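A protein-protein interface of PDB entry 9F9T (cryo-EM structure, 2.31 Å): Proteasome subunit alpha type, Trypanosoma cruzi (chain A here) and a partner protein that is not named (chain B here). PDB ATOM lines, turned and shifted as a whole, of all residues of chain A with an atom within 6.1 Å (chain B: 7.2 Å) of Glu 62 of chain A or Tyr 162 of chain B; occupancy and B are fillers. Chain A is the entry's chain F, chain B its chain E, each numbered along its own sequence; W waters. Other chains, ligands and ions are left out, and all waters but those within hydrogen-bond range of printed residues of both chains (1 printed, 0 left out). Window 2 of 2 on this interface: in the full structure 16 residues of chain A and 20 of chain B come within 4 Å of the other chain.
OD1 of Asp 118 of chain B lies within salt-bridge range of NE of Arg 83 of chain A. The guanidinium group (NH1) of Arg 83 of chain A lies within hydrogen-bond range of the backbone carbonyl oxygen (O) of Gly 160 of chain B, 3.1 Å away. O of Tyr 162 of chain B is in hydrogen-bond range of NE2 of Gln 61 of chain A, 3.2 Å away. The side-chain hydroxyl of Thr 163 of chain B is in hydrogen-bond range of the side-chain amide nitrogen of Gln 61 of chain A (3.3 Å).
SG of Cys 117 of chain B is in hydrogen-bond range of O of Ala 113 of chain B (3.3 Å). The side-chain sulfur (SG) of Cys 117 of chain B sits close to the backbone carbonyl oxygen (O) of Gly 160 of chain B, 3.6 Å away. O of Trp 154 of chain B is in hydrogen-bond range of N of Ile 143 of chain B (2.7 Å). O of Thr 163 of chain B lies within hydrogen-bond range of N of Gln 155 of chain B (2.9 Å). OG1 of Thr 161 of chain B lies within hydrogen-bond range of OG1 of Thr 163 of chain B.
Among the printed residues, pairs that only touch across the chains: Glu 62 of chain A with Tyr 162 of chain B (3.6 Å), Gln 61 of chain A with Thr 161 of chain B (3.7 Å), Tyr 60 of chain A with Trp 154 of chain B (3.7 Å), Arg 83 of chain A with Cys 117 of chain B (3.7 Å), Arg 83 of chain A with Leu 114 of chain B (3.8 Å), Arg 83 of chain A with Tyr 162 of chain B (3.8 Å) and Tyr 60 of chain A with Glu 110 of chain B (3.97 Å).
Of the printed residues of chain B, Tyr 60 of chain A touches Glu 110 (3.97 Å) and Trp 154 (3.7 Å). Printed residues of chain A within 4 Å of Glu 110 of chain B: Tyr 60. Of the printed residues of chain A, Leu 114 of chain B touches Arg 83 (3.8 Å). Of the printed residues of chain A, Gly 160 of chain B touches Arg 83. Of the printed residues of chain A, Tyr 162 of chain B touches Gln 61 (3.2 Å), Glu 62 (3.6 Å) and Arg 83 (3.8 Å). The nearest residue of chain A that does not touch Tyr 162 of chain B is Tyr 60 of chain A (5.0 Å).
Of the 21 printed residues of chain B, 9 touch a printed residue of chain A. Hydrophobic or aromatic side chains of chain B within 4 Å of the printed part of chain A: Leu 114, Trp 154 and Tyr 162. Among the printed residues, 11 pairs touch across the chains. Among the printed residues, Asp or Glu carboxylates within 4 Å of a Lys or Arg side-chain nitrogen of the other chain: Arg 83 of chain A with Asp 118 of chain B (3.9 Å).
Water W1 lies within hydrogen-bond range of O of Ser 159 of chain B (3.1 Å) and N of Val 79 of chain A (3.2 Å).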
ATOM      1  N   LYS A  50     -10.250 -14.968 -35.491  1.00  0.00           N
ATOM      2  CA  LYS A  50     -10.348 -14.011 -34.400  1.00  0.00           C
ATOM      3  C   LYS A  50     -10.826 -14.696 -33.109  1.00  0.00           C
ATOM      4  O   LYS A  50     -11.879 -15.338 -33.113  1.00  0.00           O
ATOM      5  CB  LYS A  50     -11.336 -12.905 -34.771  1.00  0.00           C
ATOM      6  CG  LYS A  50     -11.098 -12.243 -36.114  1.00  0.00           C
ATOM      7  CD  LYS A  50     -12.019 -11.038 -36.337  1.00  0.00           C
ATOM      8  CE  LYS A  50     -13.273 -11.322 -37.140  1.00  0.00           C
ATOM      9  NZ  LYS A  50     -14.049 -10.080 -37.371  1.00  0.00           N
ATOM     10  N   TYR A  60     -14.134  -8.914 -30.852  1.00  0.00           N
ATOM     11  CA  TYR A  60     -13.494  -8.240 -32.026  1.00  0.00           C
ATOM     12  C   TYR A  60     -12.033  -7.857 -31.729  1.00  0.00           C
ATOM     13  O   TYR A  60     -11.783  -6.839 -31.074  1.00  0.00           O
ATOM     14  CB  TYR A  60     -14.390  -7.049 -32.403  1.00  0.00           C
ATOM     15  CG  TYR A  60     -13.763  -5.966 -33.275  1.00  0.00           C
ATOM     16  CD1 TYR A  60     -12.938  -6.281 -34.354  1.00  0.00           C
ATOM     17  CD2 TYR A  60     -14.025  -4.620 -33.032  1.00  0.00           C
ATOM     18  CE1 TYR A  60     -12.365  -5.294 -35.143  1.00  0.00           C
ATOM     19  CE2 TYR A  60     -13.468  -3.624 -33.819  1.00  0.00           C
ATOM     20  CZ  TYR A  60     -12.634  -3.961 -34.873  1.00  0.00           C
ATOM     21  OH  TYR A  60     -12.092  -2.975 -35.645  1.00  0.00           O
ATOM     22  N   GLN A  61     -11.080  -8.664 -32.241  1.00  0.00           N
ATOM     23  CA  GLN A  61      -9.640  -8.395 -32.152  1.00  0.00           C
ATOM     24  C   GLN A  61      -9.009  -8.225 -33.536  1.00  0.00           C
ATOM     25  O   GLN A  61      -8.967  -9.164 -34.331  1.00  0.00           O
ATOM     26  CB  GLN A  61      -8.904  -9.528 -31.430  1.00  0.00           C
ATOM     27  CG  GLN A  61      -8.706  -9.290 -29.932  1.00  0.00           C
ATOM     28  CD  GLN A  61      -7.381  -8.645 -29.609  1.00  0.00           C
ATOM     29  OE1 GLN A  61      -6.338  -9.298 -29.599  1.00  0.00           O
ATOM     30  NE2 GLN A  61      -7.414  -7.358 -29.304  1.00  0.00           N
ATOM     31  N   GLU A  62      -8.512  -7.012 -33.805  1.00  0.00           N
ATOM     32  CA  GLU A  62      -7.618  -6.739 -34.927  1.00  0.00           C
ATOM     33  C   GLU A  62      -6.518  -7.799 -34.986  1.00  0.00           C
ATOM     34  O   GLU A  62      -5.681  -7.878 -34.087  1.00  0.00           O
ATOM     35  CB  GLU A  62      -6.919  -5.378 -34.773  1.00  0.00           C
ATOM     36  CG  GLU A  62      -7.616  -4.204 -35.463  1.00  0.00           C
ATOM     37  CD  GLU A  62      -6.808  -2.908 -35.528  1.00  0.00           C
ATOM     38  OE1 GLU A  62      -5.881  -2.726 -34.694  1.00  0.00           O
ATOM     39  OE2 GLU A  62      -7.087  -2.088 -36.437  1.00  0.00           O
ATOM     40  N   LYS A  63      -6.522  -8.574 -36.065  1.00  0.00           N
ATOM     41  CA  LYS A  63      -5.485  -9.551 -36.318  1.00  0.00           C
ATOM     42  C   LYS A  63      -4.901  -9.434 -37.738  1.00  0.00           C
ATOM     43  O   LYS A  63      -3.947 -10.135 -38.050  1.00  0.00           O
ATOM     44  CB  LYS A  63      -6.114 -10.922 -36.061  1.00  0.00           C
ATOM     45  CG  LYS A  63      -5.161 -12.067 -35.766  1.00  0.00           C
ATOM     46  CD  LYS A  63      -5.883 -13.398 -35.670  1.00  0.00           C
ATOM     47  CE  LYS A  63      -4.972 -14.612 -35.613  1.00  0.00           C
ATOM     48  NZ  LYS A  63      -4.029 -14.539 -34.470  1.00  0.00           N
ATOM     49  N   VAL A  64      -5.454  -8.556 -38.584  1.00  0.00           N
ATOM     50  CA  VAL A  64      -5.041  -8.375 -39.962  1.00  0.00           C
ATOM     51  C   VAL A  64      -4.886  -6.872 -40.197  1.00  0.00           C
ATOM     52  O   VAL A  64      -5.758  -6.102 -39.835  1.00  0.00           O
ATOM     53  CB  VAL A  64      -6.055  -9.031 -40.903  1.00  0.00           C
ATOM     54  CG1 VAL A  64      -5.668  -8.951 -42.338  1.00  0.00           C
ATOM     55  CG2 VAL A  64      -6.252 -10.500 -40.598  1.00  0.00           C
ATOM     56  N   PHE A  65      -3.719  -6.437 -40.690  1.00  0.00           N
ATOM     57  CA  PHE A  65      -3.452  -5.025 -40.923  1.00  0.00           C
ATOM     58  C   PHE A  65      -3.004  -4.810 -42.374  1.00  0.00           C
ATOM     59  O   PHE A  65      -2.340  -5.662 -42.976  1.00  0.00           O
ATOM     60  CB  PHE A  65      -2.262  -4.522 -40.109  1.00  0.00           C
ATOM     61  CG  PHE A  65      -2.429  -4.675 -38.635  1.00  0.00           C
ATOM     62  CD1 PHE A  65      -2.600  -3.567 -37.827  1.00  0.00           C
ATOM     63  CD2 PHE A  65      -2.429  -5.930 -38.054  1.00  0.00           C
ATOM     64  CE1 PHE A  65      -2.796  -3.702 -36.459  1.00  0.00           C
ATOM     65  CE2 PHE A  65      -2.660  -6.069 -36.693  1.00  0.00           C
ATOM     66  CZ  PHE A  65      -2.866  -4.958 -35.898  1.00  0.00           C
ATOM     67  N   ILE A  75      -1.141 -11.235 -37.817  1.00  0.00           N
ATOM     68  CA  ILE A  75      -0.303 -11.510 -36.665  1.00  0.00           C
ATOM     69  C   ILE A  75      -0.779 -12.710 -35.838  1.00  0.00           C
ATOM     70  O   ILE A  75      -1.879 -13.216 -36.034  1.00  0.00           O
ATOM     71  CB  ILE A  75      -0.187 -10.291 -35.779  1.00  0.00           C
ATOM     72  CG1 ILE A  75      -1.490  -9.994 -35.014  1.00  0.00           C
ATOM     73  CG2 ILE A  75       0.292  -9.099 -36.603  1.00  0.00           C
ATOM     74  CD1 ILE A  75      -1.539  -8.593 -34.325  1.00  0.00           C
ATOM     75  N   VAL A  79       0.018  -8.482 -29.390  1.00  0.00           N
ATOM     76  CA  VAL A  79      -0.554  -7.563 -30.321  1.00  0.00           C
ATOM     77  C   VAL A  79       0.173  -6.233 -30.238  1.00  0.00           C
ATOM     78  O   VAL A  79       0.264  -5.504 -31.227  1.00  0.00           O
ATOM     79  CB  VAL A  79      -2.061  -7.468 -30.037  1.00  0.00           C
ATOM     80  CG1 VAL A  79      -2.733  -6.369 -30.830  1.00  0.00           C
ATOM     81  CG2 VAL A  79      -2.715  -8.830 -30.305  1.00  0.00           C
ATOM     82  N   ARG A  83       1.542  -4.152 -33.438  1.00  0.00           N
ATOM     83  CA  ARG A  83       1.202  -2.803 -33.841  1.00  0.00           C
ATOM     84  C   ARG A  83       2.461  -1.995 -34.092  1.00  0.00           C
ATOM     85  O   ARG A  83       2.404  -0.937 -34.718  1.00  0.00           O
ATOM     86  CB  ARG A  83       0.287  -2.079 -32.835  1.00  0.00           C
ATOM     87  CG  ARG A  83      -1.126  -2.627 -32.850  1.00  0.00           C
ATOM     88  CD  ARG A  83      -2.092  -1.576 -32.325  1.00  0.00           C
ATOM     89  NE  ARG A  83      -1.702  -1.098 -31.004  1.00  0.00           N
ATOM     90  CZ  ARG A  83      -1.976  -1.750 -29.878  1.00  0.00           C
ATOM     91  NH1 ARG A  83      -1.323  -1.465 -28.759  1.00  0.00           N
ATOM     92  NH2 ARG A  83      -2.857  -2.738 -29.910  1.00  0.00           N
ATOM     93  N   VAL B 109     -14.000   6.927 -30.486  1.00  0.00           N
ATOM     94  CA  VAL B 109     -13.759   6.185 -29.272  1.00  0.00           C
ATOM     95  C   VAL B 109     -12.702   5.117 -29.484  1.00  0.00           C
ATOM     96  O   VAL B 109     -11.914   4.828 -28.593  1.00  0.00           O
ATOM     97  CB  VAL B 109     -15.042   5.477 -28.819  1.00  0.00           C
ATOM     98  CG1 VAL B 109     -14.715   4.636 -27.604  1.00  0.00           C
ATOM     99  CG2 VAL B 109     -16.233   6.417 -28.548  1.00  0.00           C
ATOM    100  N   GLU B 110     -12.758   4.418 -30.600  1.00  0.00           N
ATOM    101  CA  GLU B 110     -11.732   3.444 -30.873  1.00  0.00           C
ATOM    102  C   GLU B 110     -10.383   4.121 -30.988  1.00  0.00           C
ATOM    103  O   GLU B 110      -9.407   3.625 -30.502  1.00  0.00           O
ATOM    104  CB  GLU B 110     -12.089   2.662 -32.122  1.00  0.00           C
ATOM    105  CG  GLU B 110     -11.250   1.430 -32.379  1.00  0.00           C
ATOM    106  CD  GLU B 110     -11.494   0.824 -33.767  1.00  0.00           C
ATOM    107  OE1 GLU B 110     -12.697   0.647 -34.128  1.00  0.00           O
ATOM    108  OE2 GLU B 110     -10.489   0.516 -34.492  1.00  0.00           O
ATOM    109  N   SER B 111     -10.283   5.269 -31.601  1.00  0.00           N
ATOM    110  CA  SER B 111      -8.955   5.846 -31.781  1.00  0.00           C
ATOM    111  C   SER B 111      -8.326   6.190 -30.432  1.00  0.00           C
ATOM    112  O   SER B 111      -7.110   6.159 -30.275  1.00  0.00           O
ATOM    113  CB  SER B 111      -9.031   7.092 -32.605  1.00  0.00           C
ATOM    114  OG  SER B 111     -10.340   7.332 -33.049  1.00  0.00           O
ATOM    115  N   CYS B 112      -9.191   6.624 -29.502  1.00  0.00           N
ATOM    116  CA  CYS B 112      -8.833   7.010 -28.163  1.00  0.00           C
ATOM    117  C   CYS B 112      -8.322   5.795 -27.388  1.00  0.00           C
ATOM    118  O   CYS B 112      -7.279   5.846 -26.744  1.00  0.00           O
ATOM    119  CB  CYS B 112     -10.050   7.653 -27.522  1.00  0.00           C
ATOM    120  SG  CYS B 112      -9.711   8.306 -25.862  1.00  0.00           S
ATOM    121  N   ALA B 113      -9.011   4.665 -27.486  1.00  0.00           N
ATOM    122  CA  ALA B 113      -8.509   3.440 -26.887  1.00  0.00           C
ATOM    123  C   ALA B 113      -7.196   3.000 -27.517  1.00  0.00           C
ATOM    124  O   ALA B 113      -6.295   2.535 -26.839  1.00  0.00           O
ATOM    125  CB  ALA B 113      -9.545   2.352 -26.967  1.00  0.00           C
ATOM    126  N   LEU B 114      -7.065   3.153 -28.822  1.00  0.00           N
ATOM    127  CA  LEU B 114      -5.817   2.837 -29.488  1.00  0.00           C
ATOM    128  C   LEU B 114      -4.686   3.709 -28.953  1.00  0.00           C
ATOM    129  O   LEU B 114      -3.576   3.235 -28.780  1.00  0.00           O
ATOM    130  CB  LEU B 114      -6.023   3.035 -30.995  1.00  0.00           C
ATOM    131  CG  LEU B 114      -4.755   3.019 -31.866  1.00  0.00           C
ATOM    132  CD1 LEU B 114      -4.102   1.647 -31.882  1.00  0.00           C
ATOM    133  CD2 LEU B 114      -5.091   3.466 -33.287  1.00  0.00           C
ATOM    134  N   ALA B 115      -4.961   5.001 -28.752  1.00  0.00           N
ATOM    135  CA  ALA B 115      -3.918   5.947 -28.388  1.00  0.00           C
ATOM    136  C   ALA B 115      -3.430   5.670 -26.956  1.00  0.00           C
ATOM    137  O   ALA B 115      -2.253   5.835 -26.645  1.00  0.00           O
ATOM    138  CB  ALA B 115      -4.406   7.384 -28.566  1.00  0.00           C
ATOM    139  N   CYS B 117      -3.395   2.794 -25.449  1.00  0.00           N
ATOM    140  CA  CYS B 117      -2.657   1.543 -25.465  1.00  0.00           C
ATOM    141  C   CYS B 117      -1.260   1.658 -26.018  1.00  0.00           C
ATOM    142  O   CYS B 117      -0.407   0.833 -25.695  1.00  0.00           O
ATOM    143  CB  CYS B 117      -3.368   0.507 -26.312  1.00  0.00           C
ATOM    144  SG  CYS B 117      -4.821  -0.060 -25.400  1.00  0.00           S
ATOM    145  N   ASP B 118      -1.029   2.629 -26.890  1.00  0.00           N
ATOM    146  CA  ASP B 118       0.312   2.770 -27.410  1.00  0.00           C
ATOM    147  C   ASP B 118       1.212   3.009 -26.194  1.00  0.00           C
ATOM    148  O   ASP B 118       2.196   2.295 -26.025  1.00  0.00           O
ATOM    149  CB  ASP B 118       0.376   3.823 -28.530  1.00  0.00           C
ATOM    150  CG  ASP B 118      -0.155   3.364 -29.892  1.00  0.00           C
ATOM    151  OD1 ASP B 118       0.178   2.220 -30.312  1.00  0.00           O
ATOM    152  OD2 ASP B 118      -0.882   4.166 -30.545  1.00  0.00           O
ATOM    153  N   ILE B 143     -13.389   2.550 -21.656  1.00  0.00           N
ATOM    154  CA  ILE B 143     -13.790   3.797 -22.284  1.00  0.00           C
ATOM    155  C   ILE B 143     -15.141   3.570 -22.932  1.00  0.00           C
ATOM    156  O   ILE B 143     -15.385   2.549 -23.537  1.00  0.00           O
ATOM    157  CB  ILE B 143     -12.709   4.258 -23.278  1.00  0.00           C
ATOM    158  CG1 ILE B 143     -11.368   4.484 -22.575  1.00  0.00           C
ATOM    159  CG2 ILE B 143     -13.164   5.507 -23.999  1.00  0.00           C
ATOM    160  CD1 ILE B 143     -10.186   4.118 -23.395  1.00  0.00           C
ATOM    161  N   TRP B 154     -15.117   0.200 -24.906  1.00  0.00           N
ATOM    162  CA  TRP B 154     -13.845  -0.451 -25.098  1.00  0.00           C
ATOM    163  C   TRP B 154     -13.085  -0.614 -23.812  1.00  0.00           C
ATOM    164  O   TRP B 154     -13.260   0.147 -22.903  1.00  0.00           O
ATOM    165  CB  TRP B 154     -12.986   0.339 -26.077  1.00  0.00           C
ATOM    166  CG  TRP B 154     -13.651   0.442 -27.412  1.00  0.00           C
ATOM    167  CD1 TRP B 154     -14.737   1.201 -27.736  1.00  0.00           C
ATOM    168  CD2 TRP B 154     -13.235  -0.206 -28.608  1.00  0.00           C
ATOM    169  NE1 TRP B 154     -15.027   1.045 -29.062  1.00  0.00           N
ATOM    170  CE2 TRP B 154     -14.108   0.209 -29.616  1.00  0.00           C
ATOM    171  CE3 TRP B 154     -12.216  -1.081 -28.899  1.00  0.00           C
ATOM    172  CZ2 TRP B 154     -14.001  -0.225 -30.923  1.00  0.00           C
ATOM    173  CZ3 TRP B 154     -12.089  -1.517 -30.201  1.00  0.00           C
ATOM    174  CH2 TRP B 154     -12.958  -1.071 -31.203  1.00  0.00           C
ATOM    175  N   GLN B 155     -12.214  -1.612 -23.803  1.00  0.00           N
ATOM    176  CA  GLN B 155     -11.418  -1.966 -22.650  1.00  0.00           C
ATOM    177  C   GLN B 155      -9.975  -2.166 -23.076  1.00  0.00           C
ATOM    178  O   GLN B 155      -9.686  -2.954 -23.970  1.00  0.00           O
ATOM    179  CB  GLN B 155     -11.804  -3.290 -22.002  1.00  0.00           C
ATOM    180  CG  GLN B 155     -10.779  -3.626 -20.925  1.00  0.00           C
ATOM    181  CD  GLN B 155     -10.745  -5.067 -20.493  1.00  0.00           C
ATOM    182  OE1 GLN B 155      -9.736  -5.760 -20.601  1.00  0.00           O
ATOM    183  NE2 GLN B 155     -11.861  -5.519 -19.964  1.00  0.00           N
ATOM    184  N   THR B 156      -9.102  -1.496 -22.333  1.00  0.00           N
ATOM    185  CA  THR B 156      -7.668  -1.594 -22.496  1.00  0.00           C
ATOM    186  C   THR B 156      -7.115  -2.258 -21.259  1.00  0.00           C
ATOM    187  O   THR B 156      -7.698  -2.027 -20.205  1.00  0.00           O
ATOM    188  CB  THR B 156      -6.965  -0.236 -22.480  1.00  0.00           C
ATOM    189  OG1 THR B 156      -6.402  -0.094 -21.169  1.00  0.00           O
ATOM    190  CG2 THR B 156      -7.874   0.910 -22.889  1.00  0.00           C
ATOM    191  N   ASP B 157      -5.964  -2.944 -21.406  1.00  0.00           N
ATOM    192  CA  ASP B 157      -5.310  -3.626 -20.307  1.00  0.00           C
ATOM    193  C   ASP B 157      -3.788  -3.441 -20.364  1.00  0.00           C
ATOM    194  O   ASP B 157      -3.253  -2.912 -21.332  1.00  0.00           O
ATOM    195  CB  ASP B 157      -5.827  -5.055 -20.270  1.00  0.00           C
ATOM    196  CG  ASP B 157      -4.977  -6.032 -21.052  1.00  0.00           C
ATOM    197  OD1 ASP B 157      -3.860  -5.644 -21.468  1.00  0.00           O
ATOM    198  OD2 ASP B 157      -5.435  -7.202 -21.212  1.00  0.00           O
ATOM    199  N   SER B 159      -1.223  -5.219 -21.127  1.00  0.00           N
ATOM    200  CA  SER B 159      -0.570  -5.773 -22.311  1.00  0.00           C
ATOM    201  C   SER B 159      -0.590  -4.785 -23.457  1.00  0.00           C
ATOM    202  O   SER B 159       0.190  -4.920 -24.381  1.00  0.00           O
ATOM    203  CB  SER B 159      -1.178  -7.074 -22.788  1.00  0.00           C
ATOM    204  OG  SER B 159      -2.582  -7.060 -22.708  1.00  0.00           O
ATOM    205  N   GLY B 160      -1.490  -3.817 -23.410  1.00  0.00           N
ATOM    206  CA  GLY B 160      -1.701  -2.916 -24.530  1.00  0.00           C
ATOM    207  C   GLY B 160      -2.699  -3.511 -25.520  1.00  0.00           C
ATOM    208  O   GLY B 160      -2.958  -2.880 -26.532  1.00  0.00           O
ATOM    209  N   THR B 161      -3.264  -4.700 -25.245  1.00  0.00           N
ATOM    210  CA  THR B 161      -4.431  -5.059 -26.021  1.00  0.00           C
ATOM    211  C   THR B 161      -5.582  -4.134 -25.660  1.00  0.00           C
ATOM    212  O   THR B 161      -5.700  -3.715 -24.522  1.00  0.00           O
ATOM    213  CB  THR B 161      -4.942  -6.509 -26.003  1.00  0.00           C
ATOM    214  OG1 THR B 161      -6.359  -6.305 -25.967  1.00  0.00           O
ATOM    215  CG2 THR B 161      -4.506  -7.410 -24.878  1.00  0.00           C
ATOM    216  N   TYR B 162      -6.376  -3.783 -26.674  1.00  0.00           N
ATOM    217  CA  TYR B 162      -7.646  -3.133 -26.448  1.00  0.00           C
ATOM    218  C   TYR B 162      -8.702  -3.882 -27.234  1.00  0.00           C
ATOM    219  O   TYR B 162      -8.372  -4.560 -28.198  1.00  0.00           O
ATOM    220  CB  TYR B 162      -7.636  -1.643 -26.791  1.00  0.00           C
ATOM    221  CG  TYR B 162      -7.557  -1.313 -28.262  1.00  0.00           C
ATOM    222  CD1 TYR B 162      -8.675  -0.877 -28.968  1.00  0.00           C
ATOM    223  CD2 TYR B 162      -6.342  -1.396 -28.946  1.00  0.00           C
ATOM    224  CE1 TYR B 162      -8.590  -0.545 -30.319  1.00  0.00           C
ATOM    225  CE2 TYR B 162      -6.249  -1.072 -30.295  1.00  0.00           C
ATOM    226  CZ  TYR B 162      -7.376  -0.657 -30.985  1.00  0.00           C
ATOM    227  OH  TYR B 162      -7.267  -0.367 -32.306  1.00  0.00           O
ATOM    228  N   THR B 163      -9.957  -3.760 -26.794  1.00  0.00           N
ATOM    229  CA  THR B 163     -10.990  -4.669 -27.236  1.00  0.00           C
ATOM    230  C   THR B 163     -12.370  -4.106 -26.963  1.00  0.00           C
ATOM    231  O   THR B 163     -12.588  -3.509 -25.916  1.00  0.00           O
ATOM    232  CB  THR B 163     -10.856  -6.006 -26.511  1.00  0.00           C
ATOM    233  OG1 THR B 163      -9.589  -6.531 -26.904  1.00  0.00           O
ATOM    234  CG2 THR B 163     -11.967  -6.968 -26.860  1.00  0.00           C
ATOM    235  N   ARG B 164     -13.297  -4.357 -27.893  1.00  0.00           N
ATOM    236  CA  ARG B 164     -14.662  -3.868 -27.774  1.00  0.00           C
ATOM    237  C   ARG B 164     -15.534  -4.950 -27.193  1.00  0.00           C
ATOM    238  O   ARG B 164     -15.356  -6.098 -27.522  1.00  0.00           O
ATOM    239  CB  ARG B 164     -15.323  -3.517 -29.103  1.00  0.00           C
ATOM    240  CG  ARG B 164     -16.718  -2.919 -28.925  1.00  0.00           C
ATOM    241  CD  ARG B 164     -17.411  -2.649 -30.262  1.00  0.00           C
ATOM    242  NE  ARG B 164     -18.732  -2.080 -30.031  1.00  0.00           N
ATOM    243  CZ  ARG B 164     -19.478  -1.471 -30.950  1.00  0.00           C
ATOM    244  NH1 ARG B 164     -19.059  -1.389 -32.203  1.00  0.00           N
ATOM    245  NH2 ARG B 164     -20.640  -0.940 -30.592  1.00  0.00           N
ATOM    246  N   TYR B 165     -16.462  -4.509 -26.337  1.00  0.00           N
ATOM    247  CA  TYR B 165     -17.249  -5.351 -25.463  1.00  0.00           C
ATOM    248  C   TYR B 165     -18.677  -4.818 -25.484  1.00  0.00           C
ATOM    249  O   TYR B 165     -18.872  -3.615 -25.649  1.00  0.00           O
ATOM    250  CB  TYR B 165     -16.644  -5.269 -24.051  1.00  0.00           C
ATOM    251  CG  TYR B 165     -15.589  -6.329 -23.766  1.00  0.00           C
ATOM    252  CD1 TYR B 165     -15.943  -7.661 -23.540  1.00  0.00           C
ATOM    253  CD2 TYR B 165     -14.239  -6.007 -23.715  1.00  0.00           C
ATOM    254  CE1 TYR B 165     -14.977  -8.643 -23.331  1.00  0.00           C
ATOM    255  CE2 TYR B 165     -13.266  -6.976 -23.469  1.00  0.00           C
ATOM    256  CZ  TYR B 165     -13.631  -8.299 -23.298  1.00  0.00           C
ATOM    257  OH  TYR B 165     -12.662  -9.249 -23.081  1.00  0.00           O
HETATM  258  O   HOH W   1       0.062  -7.274 -26.436  1.00  0.00           O
